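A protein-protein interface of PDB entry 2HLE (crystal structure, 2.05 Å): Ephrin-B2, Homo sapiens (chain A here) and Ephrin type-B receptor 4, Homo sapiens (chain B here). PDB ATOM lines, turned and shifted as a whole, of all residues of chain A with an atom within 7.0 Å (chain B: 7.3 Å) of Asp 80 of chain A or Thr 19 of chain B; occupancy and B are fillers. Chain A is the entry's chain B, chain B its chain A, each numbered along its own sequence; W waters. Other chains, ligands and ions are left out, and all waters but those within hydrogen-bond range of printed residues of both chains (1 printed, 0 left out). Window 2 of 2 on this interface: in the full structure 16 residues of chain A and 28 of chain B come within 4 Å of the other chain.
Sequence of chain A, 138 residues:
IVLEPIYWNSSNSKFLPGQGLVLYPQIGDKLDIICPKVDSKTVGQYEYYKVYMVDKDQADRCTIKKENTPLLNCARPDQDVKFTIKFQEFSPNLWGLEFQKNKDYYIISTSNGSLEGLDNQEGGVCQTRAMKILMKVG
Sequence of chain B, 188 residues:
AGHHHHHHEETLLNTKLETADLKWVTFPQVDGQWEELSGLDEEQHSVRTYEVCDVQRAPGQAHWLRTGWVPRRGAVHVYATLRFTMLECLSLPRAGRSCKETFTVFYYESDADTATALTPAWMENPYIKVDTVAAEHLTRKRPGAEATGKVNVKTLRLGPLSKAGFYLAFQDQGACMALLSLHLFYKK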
ATOM      1  N   TYR A   7      12.473 -16.230 -23.720  1.00  0.00           N
ATOM      2  CA  TYR A   7      11.743 -17.381 -23.200  1.00  0.00           C
ATOM      3  C   TYR A   7      10.258 -17.152 -23.368  1.00  0.00           C
ATOM      4  O   TYR A   7       9.687 -16.161 -22.831  1.00  0.00           O
ATOM      5  CB  TYR A   7      12.097 -17.634 -21.734  1.00  0.00           C
ATOM      6  CG  TYR A   7      13.533 -18.109 -21.571  1.00  0.00           C
ATOM      7  CD1 TYR A   7      13.844 -19.476 -21.514  1.00  0.00           C
ATOM      8  CD2 TYR A   7      14.588 -17.191 -21.510  1.00  0.00           C
ATOM      9  CE1 TYR A   7      15.160 -19.904 -21.372  1.00  0.00           C
ATOM     10  CE2 TYR A   7      15.899 -17.616 -21.371  1.00  0.00           C
ATOM     11  CZ  TYR A   7      16.175 -18.956 -21.295  1.00  0.00           C
ATOM     12  OH  TYR A   7      17.482 -19.357 -21.159  1.00  0.00           O
ATOM     13  N   ILE A  34      13.298 -19.541 -26.931  1.00  0.00           N
ATOM     14  CA  ILE A  34      13.297 -20.832 -26.169  1.00  0.00           C
ATOM     15  C   ILE A  34      11.983 -21.123 -25.508  1.00  0.00           C
ATOM     16  O   ILE A  34      11.452 -20.281 -24.748  1.00  0.00           O
ATOM     17  CB  ILE A  34      14.350 -20.867 -25.033  1.00  0.00           C
ATOM     18  CG1 ILE A  34      15.712 -20.430 -25.543  1.00  0.00           C
ATOM     19  CG2 ILE A  34      14.466 -22.318 -24.433  1.00  0.00           C
ATOM     20  CD1 ILE A  34      15.861 -18.949 -25.718  1.00  0.00           C
ATOM     21  N   CYS A  35      11.468 -22.318 -25.764  1.00  0.00           N
ATOM     22  CA  CYS A  35      10.380 -22.886 -24.970  1.00  0.00           C
ATOM     23  C   CYS A  35      10.989 -23.745 -23.852  1.00  0.00           C
ATOM     24  O   CYS A  35      11.615 -24.768 -24.144  1.00  0.00           O
ATOM     25  CB  CYS A  35       9.444 -23.700 -25.841  1.00  0.00           C
ATOM     26  SG  CYS A  35       8.197 -22.657 -26.616  1.00  0.00           S
ATOM     27  N   PRO A  36      10.835 -23.320 -22.576  1.00  0.00           N
ATOM     28  CA  PRO A  36      11.609 -23.940 -21.482  1.00  0.00           C
ATOM     29  C   PRO A  36      11.006 -25.223 -20.890  1.00  0.00           C
ATOM     30  O   PRO A  36       9.790 -25.428 -20.945  1.00  0.00           O
ATOM     31  CB  PRO A  36      11.671 -22.823 -20.421  1.00  0.00           C
ATOM     32  CG  PRO A  36      10.759 -21.713 -20.925  1.00  0.00           C
ATOM     33  CD  PRO A  36       9.959 -22.267 -22.056  1.00  0.00           C
ATOM     34  N   LYS A  37      11.883 -26.068 -20.347  1.00  0.00           N
ATOM     35  CA  LYS A  37      11.523 -27.373 -19.781  1.00  0.00           C
ATOM     36  C   LYS A  37      10.774 -27.151 -18.481  1.00  0.00           C
ATOM     37  O   LYS A  37      11.074 -26.183 -17.766  1.00  0.00           O
ATOM     38  CB  LYS A  37      12.823 -28.161 -19.509  1.00  0.00           C
ATOM     39  CG  LYS A  37      12.687 -29.557 -18.969  1.00  0.00           C
ATOM     40  CD  LYS A  37      14.072 -30.139 -18.706  1.00  0.00           C
ATOM     41  N   VAL A  38       9.806 -28.010 -18.159  1.00  0.00           N
ATOM     42  CA  VAL A  38       9.303 -28.016 -16.775  1.00  0.00           C
ATOM     43  C   VAL A  38      10.259 -28.871 -15.930  1.00  0.00           C
ATOM     44  O   VAL A  38      10.321 -30.101 -16.051  1.00  0.00           O
ATOM     45  CB  VAL A  38       7.810 -28.416 -16.627  1.00  0.00           C
ATOM     46  CG1 VAL A  38       6.933 -27.362 -17.304  1.00  0.00           C
ATOM     47  CG2 VAL A  38       7.530 -29.829 -17.158  1.00  0.00           C
ATOM     48  N   ASP A  39      11.035 -28.178 -15.104  1.00  0.00           N
ATOM     49  CA  ASP A  39      12.163 -28.771 -14.397  1.00  0.00           C
ATOM     50  C   ASP A  39      11.733 -29.159 -12.970  1.00  0.00           C
ATOM     51  O   ASP A  39      10.540 -29.389 -12.730  1.00  0.00           O
ATOM     52  CB  ASP A  39      13.375 -27.814 -14.447  1.00  0.00           C
ATOM     53  CG  ASP A  39      13.026 -26.379 -14.046  1.00  0.00           C
ATOM     54  OD1 ASP A  39      12.744 -25.554 -14.957  1.00  0.00           O
ATOM     55  OD2 ASP A  39      13.039 -26.071 -12.829  1.00  0.00           O
ATOM     56  N   TYR A  46       3.079 -27.096 -17.888  1.00  0.00           N
ATOM     57  CA  TYR A  46       3.912 -26.748 -19.033  1.00  0.00           C
ATOM     58  C   TYR A  46       2.988 -25.919 -19.935  1.00  0.00           C
ATOM     59  O   TYR A  46       1.782 -26.132 -19.904  1.00  0.00           O
ATOM     60  CB  TYR A  46       4.436 -28.021 -19.724  1.00  0.00           C
ATOM     61  CG  TYR A  46       5.212 -27.791 -21.012  1.00  0.00           C
ATOM     62  CD1 TYR A  46       6.455 -27.168 -21.014  1.00  0.00           C
ATOM     63  CD2 TYR A  46       4.698 -28.215 -22.221  1.00  0.00           C
ATOM     64  CE1 TYR A  46       7.162 -26.971 -22.227  1.00  0.00           C
ATOM     65  CE2 TYR A  46       5.368 -28.018 -23.403  1.00  0.00           C
ATOM     66  CZ  TYR A  46       6.607 -27.397 -23.423  1.00  0.00           C
ATOM     67  OH  TYR A  46       7.260 -27.259 -24.657  1.00  0.00           O
ATOM     68  N   ARG A  76       6.482 -30.306 -25.528  1.00  0.00           N
ATOM     69  CA  ARG A  76       7.476 -31.226 -24.981  1.00  0.00           C
ATOM     70  C   ARG A  76       7.914 -30.673 -23.626  1.00  0.00           C
ATOM     71  O   ARG A  76       8.838 -29.862 -23.551  1.00  0.00           O
ATOM     72  CB  ARG A  76       8.675 -31.348 -25.935  1.00  0.00           C
ATOM     73  N   PRO A  77       7.182 -31.022 -22.564  1.00  0.00           N
ATOM     74  CA  PRO A  77       7.581 -30.684 -21.192  1.00  0.00           C
ATOM     75  C   PRO A  77       8.998 -31.082 -20.740  1.00  0.00           C
ATOM     76  O   PRO A  77       9.633 -30.303 -20.018  1.00  0.00           O
ATOM     77  CB  PRO A  77       6.537 -31.398 -20.338  1.00  0.00           C
ATOM     78  CG  PRO A  77       5.323 -31.538 -21.247  1.00  0.00           C
ATOM     79  CD  PRO A  77       5.860 -31.683 -22.625  1.00  0.00           C
ATOM     80  N   ASP A  78       9.490 -32.255 -21.144  1.00  0.00           N
ATOM     81  CA  ASP A  78      10.774 -32.763 -20.630  1.00  0.00           C
ATOM     82  C   ASP A  78      12.018 -32.329 -21.436  1.00  0.00           C
ATOM     83  O   ASP A  78      13.102 -32.878 -21.256  1.00  0.00           O
ATOM     84  CB  ASP A  78      10.731 -34.281 -20.490  1.00  0.00           C
ATOM     85  CG  ASP A  78      11.732 -34.801 -19.461  1.00  0.00           C
ATOM     86  OD1 ASP A  78      12.190 -33.994 -18.621  1.00  0.00           O
ATOM     87  OD2 ASP A  78      12.067 -36.007 -19.496  1.00  0.00           O
ATOM     88  N   GLN A  79      11.875 -31.289 -22.265  1.00  0.00           N
ATOM     89  CA  GLN A  79      12.942 -30.891 -23.175  1.00  0.00           C
ATOM     90  C   GLN A  79      12.922 -29.382 -23.465  1.00  0.00           C
ATOM     91  O   GLN A  79      11.863 -28.803 -23.739  1.00  0.00           O
ATOM     92  CB  GLN A  79      12.812 -31.699 -24.468  1.00  0.00           C
ATOM     93  CG  GLN A  79      14.041 -31.661 -25.338  1.00  0.00           C
ATOM     94  CD  GLN A  79      13.885 -32.504 -26.587  1.00  0.00           C
ATOM     95  OE1 GLN A  79      13.937 -33.739 -26.538  1.00  0.00           O
ATOM     96  NE2 GLN A  79      13.708 -31.833 -27.726  1.00  0.00           N
ATOM     97  N   ASP A  80      14.084 -28.744 -23.368  1.00  0.00           N
ATOM     98  CA  ASP A  80      14.212 -27.327 -23.713  1.00  0.00           C
ATOM     99  C   ASP A  80      14.191 -27.301 -25.254  1.00  0.00           C
ATOM    100  O   ASP A  80      15.079 -27.888 -25.878  1.00  0.00           O
ATOM    101  CB  ASP A  80      15.536 -26.715 -23.157  1.00  0.00           C
ATOM    102  CG  ASP A  80      15.329 -25.729 -21.969  1.00  0.00           C
ATOM    103  OD1 ASP A  80      14.899 -26.130 -20.861  1.00  0.00           O
ATOM    104  OD2 ASP A  80      15.643 -24.531 -22.135  1.00  0.00           O
ATOM    105  N   VAL A  81      13.164 -26.676 -25.844  1.00  0.00           N
ATOM    106  CA  VAL A  81      12.972 -26.557 -27.296  1.00  0.00           C
ATOM    107  C   VAL A  81      13.257 -25.111 -27.709  1.00  0.00           C
ATOM    108  O   VAL A  81      12.753 -24.171 -27.069  1.00  0.00           O
ATOM    109  CB  VAL A  81      11.499 -26.831 -27.741  1.00  0.00           C
ATOM    110  CG1 VAL A  81      11.316 -26.461 -29.232  1.00  0.00           C
ATOM    111  CG2 VAL A  81      11.022 -28.300 -27.464  1.00  0.00           C
ATOM    112  N   LYS A  82      13.950 -24.950 -28.831  1.00  0.00           N
ATOM    113  CA  LYS A  82      14.608 -23.698 -29.247  1.00  0.00           C
ATOM    114  C   LYS A  82      14.555 -23.443 -30.767  1.00  0.00           C
ATOM    115  O   LYS A  82      14.641 -24.385 -31.551  1.00  0.00           O
ATOM    116  CB  LYS A  82      16.067 -23.790 -28.834  1.00  0.00           C
ATOM    117  CG  LYS A  82      16.902 -22.552 -29.014  1.00  0.00           C
ATOM    118  CD  LYS A  82      18.394 -22.876 -28.755  1.00  0.00           C
ATOM    119  CE  LYS A  82      18.867 -22.535 -27.343  1.00  0.00           C
ATOM    120  NZ  LYS A  82      18.651 -23.596 -26.281  1.00  0.00           N
ATOM    121  N   PHE A  83      14.458 -22.171 -31.180  1.00  0.00           N
ATOM    122  CA  PHE A  83      14.706 -21.810 -32.577  1.00  0.00           C
ATOM    123  C   PHE A  83      15.727 -20.726 -32.536  1.00  0.00           C
ATOM    124  O   PHE A  83      15.589 -19.777 -31.736  1.00  0.00           O
ATOM    125  CB  PHE A  83      13.438 -21.293 -33.326  1.00  0.00           C
ATOM    126  CG  PHE A  83      13.617 -21.203 -34.869  1.00  0.00           C
ATOM    127  CD1 PHE A  83      13.319 -22.273 -35.682  1.00  0.00           C
ATOM    128  CD2 PHE A  83      14.101 -20.039 -35.460  1.00  0.00           C
ATOM    129  CE1 PHE A  83      13.455 -22.179 -37.047  1.00  0.00           C
ATOM    130  CE2 PHE A  83      14.281 -19.934 -36.785  1.00  0.00           C
ATOM    131  CZ  PHE A  83      13.957 -21.007 -37.613  1.00  0.00           C
ATOM    132  N   THR B  15      21.604 -35.150 -36.418  1.00  0.00           N
ATOM    133  CA  THR B  15      21.387 -33.710 -36.147  1.00  0.00           C
ATOM    134  C   THR B  15      19.900 -33.331 -36.119  1.00  0.00           C
ATOM    135  O   THR B  15      19.541 -32.406 -35.405  1.00  0.00           O
ATOM    136  CB  THR B  15      22.070 -32.839 -37.217  1.00  0.00           C
ATOM    137  OG1 THR B  15      21.443 -33.063 -38.483  1.00  0.00           O
ATOM    138  CG2 THR B  15      23.598 -33.135 -37.303  1.00  0.00           C
ATOM    139  N   LYS B  16      19.059 -34.001 -36.920  1.00  0.00           N
ATOM    140  CA  LYS B  16      17.572 -33.746 -36.936  1.00  0.00           C
ATOM    141  C   LYS B  16      16.924 -33.898 -35.554  1.00  0.00           C
ATOM    142  O   LYS B  16      16.041 -33.116 -35.173  1.00  0.00           O
ATOM    143  CB  LYS B  16      16.820 -34.727 -37.864  1.00  0.00           C
ATOM    144  CG  LYS B  16      16.675 -34.264 -39.306  1.00  0.00           C
ATOM    145  CD  LYS B  16      15.767 -35.174 -40.148  1.00  0.00           C
ATOM    146  CE  LYS B  16      16.176 -36.636 -40.053  1.00  0.00           C
ATOM    147  NZ  LYS B  16      15.755 -37.388 -41.273  1.00  0.00           N
ATOM    148  N   LEU B  17      17.344 -34.928 -34.826  1.00  0.00           N
ATOM    149  CA  LEU B  17      16.854 -35.152 -33.471  1.00  0.00           C
ATOM    150  C   LEU B  17      17.838 -34.583 -32.443  1.00  0.00           C
ATOM    151  O   LEU B  17      18.434 -35.328 -31.633  1.00  0.00           O
ATOM    152  CB  LEU B  17      16.548 -36.638 -33.246  1.00  0.00           C
ATOM    153  CG  LEU B  17      15.613 -37.275 -34.301  1.00  0.00           C
ATOM    154  CD1 LEU B  17      15.068 -38.582 -33.815  1.00  0.00           C
ATOM    155  CD2 LEU B  17      14.456 -36.377 -34.724  1.00  0.00           C
ATOM    156  N   GLU B  18      17.997 -33.254 -32.560  1.00  0.00           N
ATOM    157  CA  GLU B  18      18.610 -32.342 -31.592  1.00  0.00           C
ATOM    158  C   GLU B  18      17.878 -30.995 -31.575  1.00  0.00           C
ATOM    159  O   GLU B  18      17.740 -30.350 -32.624  1.00  0.00           O
ATOM    160  CB  GLU B  18      20.055 -32.034 -31.962  1.00  0.00           C
ATOM    161  CG  GLU B  18      20.763 -31.230 -30.888  1.00  0.00           C
ATOM    162  CD  GLU B  18      22.106 -30.749 -31.327  1.00  0.00           C
ATOM    163  OE1 GLU B  18      22.151 -30.080 -32.379  1.00  0.00           O
ATOM    164  OE2 GLU B  18      23.108 -31.040 -30.628  1.00  0.00           O
ATOM    165  N   THR B  19      17.480 -30.547 -30.379  1.00  0.00           N
ATOM    166  CA  THR B  19      16.724 -29.295 -30.194  1.00  0.00           C
ATOM    167  C   THR B  19      17.543 -28.139 -29.554  1.00  0.00           C
ATOM    168  O   THR B  19      16.979 -27.081 -29.206  1.00  0.00           O
ATOM    169  CB  THR B  19      15.425 -29.554 -29.357  1.00  0.00           C
ATOM    170  OG1 THR B  19      14.321 -29.846 -30.232  1.00  0.00           O
ATOM    171  N   ALA B  20      18.858 -28.348 -29.416  1.00  0.00           N
ATOM    172  CA  ALA B  20      19.828 -27.332 -28.954  1.00  0.00           C
ATOM    173  C   ALA B  20      20.959 -27.141 -29.970  1.00  0.00           C
ATOM    174  O   ALA B  20      21.028 -27.851 -30.965  1.00  0.00           O
ATOM    175  CB  ALA B  20      20.415 -27.758 -27.643  1.00  0.00           C
ATOM    176  N   ASP B  21      21.877 -26.214 -29.706  1.00  0.00           N
ATOM    177  CA  ASP B  21      22.911 -25.847 -30.695  1.00  0.00           C
ATOM    178  C   ASP B  21      23.869 -26.996 -30.909  1.00  0.00           C
ATOM    179  O   ASP B  21      24.123 -27.739 -29.987  1.00  0.00           O
ATOM    180  CB  ASP B  21      23.663 -24.615 -30.258  1.00  0.00           C
ATOM    181  CG  ASP B  21      22.744 -23.485 -29.923  1.00  0.00           C
ATOM    182  OD1 ASP B  21      22.623 -22.582 -30.774  1.00  0.00           O
ATOM    183  OD2 ASP B  21      22.109 -23.525 -28.836  1.00  0.00           O
ATOM    184  N   SER B  38      18.822 -22.253 -36.969  1.00  0.00           N
ATOM    185  CA  SER B  38      17.621 -23.051 -37.221  1.00  0.00           C
ATOM    186  C   SER B  38      17.038 -22.895 -38.656  1.00  0.00           C
ATOM    187  O   SER B  38      17.099 -21.866 -39.275  1.00  0.00           O
ATOM    188  CB  SER B  38      16.539 -22.714 -36.189  1.00  0.00           C
ATOM    189  OG  SER B  38      16.933 -23.142 -34.901  1.00  0.00           O
ATOM    190  N   SER B  46      11.484 -27.838 -37.550  1.00  0.00           N
ATOM    191  CA  SER B  46      12.607 -26.961 -37.267  1.00  0.00           C
ATOM    192  C   SER B  46      13.761 -27.779 -36.812  1.00  0.00           C
ATOM    193  O   SER B  46      13.672 -28.461 -35.778  1.00  0.00           O
ATOM    194  CB  SER B  46      12.281 -25.974 -36.124  1.00  0.00           C
ATOM    195  OG  SER B  46      13.487 -25.643 -35.423  1.00  0.00           O
ATOM    196  N   VAL B  47      14.869 -27.682 -37.541  1.00  0.00           N
ATOM    197  CA  VAL B  47      16.101 -28.386 -37.155  1.00  0.00           C
ATOM    198  C   VAL B  47      17.313 -27.456 -37.224  1.00  0.00           C
ATOM    199  O   VAL B  47      17.292 -26.437 -37.888  1.00  0.00           O
ATOM    200  CB  VAL B  47      16.362 -29.629 -38.090  1.00  0.00           C
ATOM    201  CG1 VAL B  47      15.481 -30.803 -37.677  1.00  0.00           C
ATOM    202  CG2 VAL B  47      16.126 -29.224 -39.530  1.00  0.00           C
ATOM    203  N   ARG B  48      18.355 -27.854 -36.540  1.00  0.00           N
ATOM    204  CA  ARG B  48      19.724 -27.288 -36.644  1.00  0.00           C
ATOM    205  C   ARG B  48      20.381 -27.457 -37.993  1.00  0.00           C
ATOM    206  O   ARG B  48      20.567 -28.588 -38.428  1.00  0.00           O
ATOM    207  CB  ARG B  48      20.607 -28.013 -35.628  1.00  0.00           C
ATOM    208  CG  ARG B  48      20.316 -27.610 -34.232  1.00  0.00           C
ATOM    209  CD  ARG B  48      20.944 -26.236 -33.980  1.00  0.00           C
ATOM    210  NE  ARG B  48      19.942 -25.477 -33.321  1.00  0.00           N
ATOM    211  CZ  ARG B  48      19.988 -24.205 -32.954  1.00  0.00           C
ATOM    212  NH1 ARG B  48      21.051 -23.391 -33.088  1.00  0.00           N
ATOM    213  NH2 ARG B  48      18.891 -23.803 -32.374  1.00  0.00           N
HETATM  214  O   HOH W   1      16.164 -25.150 -33.501  1.00  0.00           O
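The side-chain hydroxyl of Thr 19 of chain B is in hydrogen-bond range of the side-chain amide nitrogen of Gln 79 of chain A (3.3 Å).
The guanidinium group of Arg 48 of chain B is in salt-bridge range of the side-chain carboxylate of Asp 21 of chain B (2.9 Å). The side-chain hydroxyl (OG) of Ser 38 of chain B is in hydrogen-bond range of the guanidinium group (NH2) of Arg 48 of chain B, at 3.3 Å. N of Lys 37 of chain A lies within hydrogen-bond range of OD1 of Asp 80 of chain A (3.1 Å).
Among the printed residues, merely in contact across the chains: Asp 80 of chain A with Thr 19 of chain B (3.9 Å), Lys 82 of chain A with Thr 19 of chain B (3.4 Å), Lys 82 of chain A with Asp 21 of chain B (3.7 Å), Lys 82 of chain A with Arg 48 of chain B (3.8 Å), Phe 83 of chain A with Ser 38 of chain B (3.2 Å) and Phe 83 of chain A with Ser 46 of chain B (3.4 Å).
Of the printed residues of chain B, Gln 79 of chain A touches Thr 19 (3.3 Å). Of chain B, only Thr 19 (3.9 Å) comes within 4 Å of Asp 80 of chain A. Printed residues of chain B within 4 Å of Lys 82 of chain A: Thr 19, Asp 21 and Arg 48. Thr 19 of chain B touches just these residues of chain A: Gln 79, Asp 80 and Lys 82. Of the printed residues of chain A, Ser 38 of chain B touches Phe 83 (3.2 Å). Of the printed residues of chain A, Ser 46 of chain B touches Phe 83 (3.4 Å). Of the printed residues of chain A, Arg 48 of chain B touches Lys 82. The nearest residue of chain A that does not touch Thr 19 of chain B is Val 81 of chain A (4.4 Å). The nearest printed residue of chain A that does not touch Arg 48 of chain B is Phe 83 of chain A (4.4 Å).
Along chain B the printed residues that touch a printed residue of chain A span positions 19 to 48. Of the 16 printed residues of chain A, 4 touch a printed residue of chain B. Hydrophobic or aromatic side chains of chain A within 4 Å of the printed part of chain B: Phe 83. Among the printed residues, 7 pairs touch across the chains. Among the printed residues, no Asp or Glu carboxylate lies within 4 Å of a Lys or Arg side-chain nitrogen of the other chain.
Water W1 lies within hydrogen-bond range of the side-chain hydroxyl (OG) of Ser 38 of chain B (2.6 Å), the backbone carbonyl oxygen (O) of Lys 82 of chain A (2.6 Å), the guanidinium group (NH2) of Arg 48 of chain B (3.2 Å) and the side-chain hydroxyl (OG) of Ser 46 of chain B (3.3 Å).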
